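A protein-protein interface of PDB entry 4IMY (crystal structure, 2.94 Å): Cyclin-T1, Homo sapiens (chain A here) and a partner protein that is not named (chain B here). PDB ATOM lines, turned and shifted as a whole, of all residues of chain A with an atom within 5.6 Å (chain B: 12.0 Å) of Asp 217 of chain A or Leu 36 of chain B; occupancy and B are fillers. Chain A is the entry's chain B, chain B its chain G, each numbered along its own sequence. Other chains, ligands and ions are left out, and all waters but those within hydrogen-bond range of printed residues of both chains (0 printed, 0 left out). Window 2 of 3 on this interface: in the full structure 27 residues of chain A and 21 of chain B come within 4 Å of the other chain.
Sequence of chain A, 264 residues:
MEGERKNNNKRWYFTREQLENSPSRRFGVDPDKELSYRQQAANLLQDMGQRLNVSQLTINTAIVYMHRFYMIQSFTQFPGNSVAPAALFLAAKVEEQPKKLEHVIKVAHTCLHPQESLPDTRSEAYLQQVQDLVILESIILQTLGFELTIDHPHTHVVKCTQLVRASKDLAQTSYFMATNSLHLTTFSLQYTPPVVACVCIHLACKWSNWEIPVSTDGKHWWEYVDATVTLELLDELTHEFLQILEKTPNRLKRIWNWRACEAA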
ATOM      1  N   LEU A 163      11.274 -21.143   9.366  1.00  0.00           N
ATOM      2  CA  LEU A 163      12.548 -21.604   9.898  1.00  0.00           C
ATOM      3  C   LEU A 163      12.789 -21.103  11.316  1.00  0.00           C
ATOM      4  O   LEU A 163      13.242 -21.857  12.177  1.00  0.00           O
ATOM      5  CB  LEU A 163      13.687 -21.137   8.992  1.00  0.00           C
ATOM      6  CG  LEU A 163      15.081 -21.664   9.327  1.00  0.00           C
ATOM      7  CD1 LEU A 163      15.164 -23.165   9.104  1.00  0.00           C
ATOM      8  CD2 LEU A 163      16.127 -20.931   8.504  1.00  0.00           C
ATOM      9  N   VAL A 214      20.121 -15.620  17.523  1.00  0.00           N
ATOM     10  CA  VAL A 214      21.070 -16.208  16.590  1.00  0.00           C
ATOM     11  C   VAL A 214      20.860 -17.718  16.624  1.00  0.00           C
ATOM     12  O   VAL A 214      20.646 -18.294  17.693  1.00  0.00           O
ATOM     13  CB  VAL A 214      22.523 -15.875  16.968  1.00  0.00           C
ATOM     14  CG1 VAL A 214      23.488 -16.547  16.007  1.00  0.00           C
ATOM     15  CG2 VAL A 214      22.742 -14.370  16.980  1.00  0.00           C
ATOM     16  N   SER A 215      20.908 -18.359  15.459  1.00  0.00           N
ATOM     17  CA  SER A 215      20.672 -19.800  15.380  1.00  0.00           C
ATOM     18  C   SER A 215      21.635 -20.555  16.286  1.00  0.00           C
ATOM     19  O   SER A 215      22.586 -19.974  16.812  1.00  0.00           O
ATOM     20  CB  SER A 215      20.832 -20.298  13.942  1.00  0.00           C
ATOM     21  OG  SER A 215      22.198 -20.340  13.570  1.00  0.00           O
ATOM     22  N   THR A 216      21.404 -21.855  16.447  1.00  0.00           N
ATOM     23  CA  THR A 216      22.293 -22.676  17.263  1.00  0.00           C
ATOM     24  C   THR A 216      23.600 -22.969  16.535  1.00  0.00           C
ATOM     25  O   THR A 216      24.450 -23.693  17.053  1.00  0.00           O
ATOM     26  CB  THR A 216      21.653 -24.018  17.671  1.00  0.00           C
ATOM     27  OG1 THR A 216      21.264 -24.743  16.500  1.00  0.00           O
ATOM     28  CG2 THR A 216      20.440 -23.797  18.563  1.00  0.00           C
ATOM     29  N   ASP A 217      23.752 -22.420  15.330  1.00  0.00           N
ATOM     30  CA  ASP A 217      25.016 -22.509  14.606  1.00  0.00           C
ATOM     31  C   ASP A 217      25.690 -21.144  14.452  1.00  0.00           C
ATOM     32  O   ASP A 217      26.529 -20.956  13.569  1.00  0.00           O
ATOM     33  CB  ASP A 217      24.798 -23.134  13.231  1.00  0.00           C
ATOM     34  CG  ASP A 217      24.228 -24.533  13.314  1.00  0.00           C
ATOM     35  OD1 ASP A 217      24.470 -25.214  14.334  1.00  0.00           O
ATOM     36  OD2 ASP A 217      23.538 -24.950  12.359  1.00  0.00           O
ATOM     37  N   GLY A 218      25.325 -20.194  15.306  1.00  0.00           N
ATOM     38  CA  GLY A 218      25.994 -18.906  15.332  1.00  0.00           C
ATOM     39  C   GLY A 218      25.897 -18.169  14.013  1.00  0.00           C
ATOM     40  O   GLY A 218      26.861 -17.569  13.544  1.00  0.00           O
ATOM     41  N   LYS A 219      24.716 -18.213  13.416  1.00  0.00           N
ATOM     42  CA  LYS A 219      24.454 -17.467  12.197  1.00  0.00           C
ATOM     43  C   LYS A 219      23.122 -16.729  12.327  1.00  0.00           C
ATOM     44  O   LYS A 219      22.115 -17.310  12.725  1.00  0.00           O
ATOM     45  CB  LYS A 219      24.457 -18.405  10.986  1.00  0.00           C
ATOM     46  CG  LYS A 219      25.844 -18.943  10.645  1.00  0.00           C
ATOM     47  CD  LYS A 219      25.848 -19.682   9.325  1.00  0.00           C
ATOM     48  CE  LYS A 219      27.179 -19.534   8.597  1.00  0.00           C
ATOM     49  NZ  LYS A 219      27.063 -19.968   7.170  1.00  0.00           N
ATOM     50  N   TYR A 224      20.288 -17.155   6.439  1.00  0.00           N
ATOM     51  CA  TYR A 224      19.596 -18.318   5.882  1.00  0.00           C
ATOM     52  C   TYR A 224      18.647 -17.905   4.762  1.00  0.00           C
ATOM     53  O   TYR A 224      17.909 -18.732   4.229  1.00  0.00           O
ATOM     54  CB  TYR A 224      18.812 -19.057   6.975  1.00  0.00           C
ATOM     55  CG  TYR A 224      19.686 -19.655   8.058  1.00  0.00           C
ATOM     56  CD1 TYR A 224      20.249 -20.912   7.905  1.00  0.00           C
ATOM     57  CD2 TYR A 224      19.948 -18.961   9.232  1.00  0.00           C
ATOM     58  CE1 TYR A 224      21.049 -21.458   8.881  1.00  0.00           C
ATOM     59  CE2 TYR A 224      20.749 -19.502  10.218  1.00  0.00           C
ATOM     60  CZ  TYR A 224      21.295 -20.753  10.036  1.00  0.00           C
ATOM     61  OH  TYR A 224      22.095 -21.311  11.008  1.00  0.00           O
ATOM     62  N   LEU B  36      16.658 -25.808  16.030  1.00  0.00           N
ATOM     63  CA  LEU B  36      17.726 -25.019  15.421  1.00  0.00           C
ATOM     64  C   LEU B  36      17.625 -23.544  15.804  1.00  0.00           C
ATOM     65  O   LEU B  36      18.638 -22.874  16.014  1.00  0.00           O
ATOM     66  CB  LEU B  36      17.695 -25.166  13.894  1.00  0.00           C
ATOM     67  CG  LEU B  36      18.630 -24.240  13.110  1.00  0.00           C
ATOM     68  CD1 LEU B  36      20.048 -24.337  13.630  1.00  0.00           C
ATOM     69  CD2 LEU B  36      18.603 -24.565  11.632  1.00  0.00           C
ATOM     70  N   PHE B  37      16.400 -23.041  15.892  1.00  0.00           N
ATOM     71  CA  PHE B  37      16.177 -21.649  16.258  1.00  0.00           C
ATOM     72  C   PHE B  37      15.348 -21.536  17.528  1.00  0.00           C
ATOM     73  O   PHE B  37      14.238 -22.051  17.601  1.00  0.00           O
ATOM     74  CB  PHE B  37      15.468 -20.906  15.125  1.00  0.00           C
ATOM     75  CG  PHE B  37      16.386 -20.077  14.277  1.00  0.00           C
ATOM     76  CD1 PHE B  37      16.948 -18.918  14.777  1.00  0.00           C
ATOM     77  CD2 PHE B  37      16.679 -20.450  12.974  1.00  0.00           C
ATOM     78  CE1 PHE B  37      17.794 -18.150  14.002  1.00  0.00           C
ATOM     79  CE2 PHE B  37      17.524 -19.685  12.192  1.00  0.00           C
ATOM     80  CZ  PHE B  37      18.080 -18.534  12.708  1.00  0.00           C
ATOM     81  N   ALA B  38      15.884 -20.860  18.534  1.00  0.00           N
ATOM     82  CA  ALA B  38      15.094 -20.552  19.711  1.00  0.00           C
ATOM     83  C   ALA B  38      13.924 -19.680  19.271  1.00  0.00           C
ATOM     84  O   ALA B  38      13.988 -19.015  18.240  1.00  0.00           O
ATOM     85  CB  ALA B  38      15.941 -19.851  20.765  1.00  0.00           C
ATOM     86  N   GLU B  39      12.848 -19.694  20.047  1.00  0.00           N
ATOM     87  CA  GLU B  39      11.641 -18.969  19.685  1.00  0.00           C
ATOM     88  C   GLU B  39      11.822 -17.474  19.938  1.00  0.00           C
ATOM     89  O   GLU B  39      12.306 -17.074  21.000  1.00  0.00           O
ATOM     90  CB  GLU B  39      10.458 -19.498  20.496  1.00  0.00           C
ATOM     91  CG  GLU B  39       9.166 -19.625  19.712  1.00  0.00           C
ATOM     92  CD  GLU B  39       8.117 -20.429  20.457  1.00  0.00           C
ATOM     93  OE1 GLU B  39       8.052 -20.320  21.701  1.00  0.00           O
ATOM     94  OE2 GLU B  39       7.364 -21.176  19.798  1.00  0.00           O
ATOM     95  N   PRO B  40      11.446 -16.641  18.954  1.00  0.00           N
ATOM     96  CA  PRO B  40      11.493 -15.184  19.118  1.00  0.00           C
ATOM     97  C   PRO B  40      10.905 -14.738  20.453  1.00  0.00           C
ATOM     98  O   PRO B  40       9.970 -15.361  20.952  1.00  0.00           O
ATOM     99  CB  PRO B  40      10.635 -14.686  17.958  1.00  0.00           C
ATOM    100  CG  PRO B  40      10.839 -15.705  16.895  1.00  0.00           C
ATOM    101  CD  PRO B  40      11.010 -17.026  17.601  1.00  0.00           C
ATOM    102  N   TYR B  41      11.448 -13.667  21.017  1.00  0.00           N
ATOM    103  CA  TYR B  41      11.024 -13.196  22.330  1.00  0.00           C
ATOM    104  C   TYR B  41      10.769 -11.692  22.303  1.00  0.00           C
ATOM    105  O   TYR B  41      11.461 -10.951  21.603  1.00  0.00           O
ATOM    106  CB  TYR B  41      12.091 -13.535  23.372  1.00  0.00           C
ATOM    107  CG  TYR B  41      13.494 -13.166  22.939  1.00  0.00           C
ATOM    108  CD1 TYR B  41      14.163 -13.911  21.974  1.00  0.00           C
ATOM    109  CD2 TYR B  41      14.151 -12.075  23.495  1.00  0.00           C
ATOM    110  CE1 TYR B  41      15.443 -13.577  21.571  1.00  0.00           C
ATOM    111  CE2 TYR B  41      15.432 -11.736  23.098  1.00  0.00           C
ATOM    112  CZ  TYR B  41      16.071 -12.491  22.135  1.00  0.00           C
ATOM    113  OH  TYR B  41      17.346 -12.166  21.733  1.00  0.00           O
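The backbone carbonyl oxygen (O) of Leu 36 of chain B sits at hydrogen-bond distance from the backbone NH (N) of Thr 216 of chain A (3.0 Å).
OG of Ser 215 of chain A sits close to N of Asp 217 of chain A, 3.1 Å away. OG of Ser 215 of chain A is in hydrogen-bond range of O of Lys 219 of chain A. The side-chain hydroxyl (OH) of Tyr 224 of chain A is in hydrogen-bond range of the side-chain hydroxyl (OG) of Ser 215 of chain A, at 2.7 Å.
Among the printed residues, merely in contact across the chains: Leu 163 of chain A with Phe 37 of chain B (3.8 Å), Ser 215 of chain A with Leu 36 of chain B (3.7 Å), Ser 215 of chain A with Phe 37 of chain B (3.4 Å), Asp 217 of chain A with Leu 36 of chain B (3.8 Å) and Tyr 224 of chain A with Phe 37 of chain B (3.8 Å).
Printed residues of chain B within 4 Å of Leu 163 of chain A: Phe 37 (3.8 Å). No residue of chain B comes within 4 Å of Val 214 of chain A. Ser 215 of chain A touches just these residues of chain B: Leu 36 (3.7 Å) and Phe 37 (3.4 Å). Of chain B, only Leu 36 comes within 4 Å of Thr 216 of chain A. Asp 217 of chain A touches just one residue of chain B: Leu 36. No residue of chain B comes within 4 Å of Gly 218 of chain A. No residue of chain B comes within 4 Å of Lys 219 of chain A. Printed residues of chain B within 4 Å of Tyr 224 of chain A: Phe 37. Of chain A, only Ser 215, Thr 216 and Asp 217 come within 4 Å of Leu 36 of chain B. Of the printed residues of chain A, Phe 37 of chain B touches Leu 163 (3.8 Å), Ser 215 (3.4 Å) and Tyr 224 (3.8 Å). Ala 38 of chain B touches none of the printed residues of chain A. The nearest printed residue of chain A that does not touch Leu 36 of chain B is Leu 163 of chain A (4.5 Å).
Of the 8 printed residues of chain A, 5 touch a printed residue of chain B. Hydrophobic or aromatic side chains of chain A within 4 Å of the printed part of chain B: Tyr 224. Hydrophobic or aromatic side chains of chain B within 4 Å of the printed part of chain A: Leu 36 and Phe 37. Along chain B the printed residues that touch a printed residue of chain A span positions 36 to 37. Among the printed residues, no Asp or Glu carboxylate lies within 4 Å of a Lys or Arg side-chain nitrogen of the other chain.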
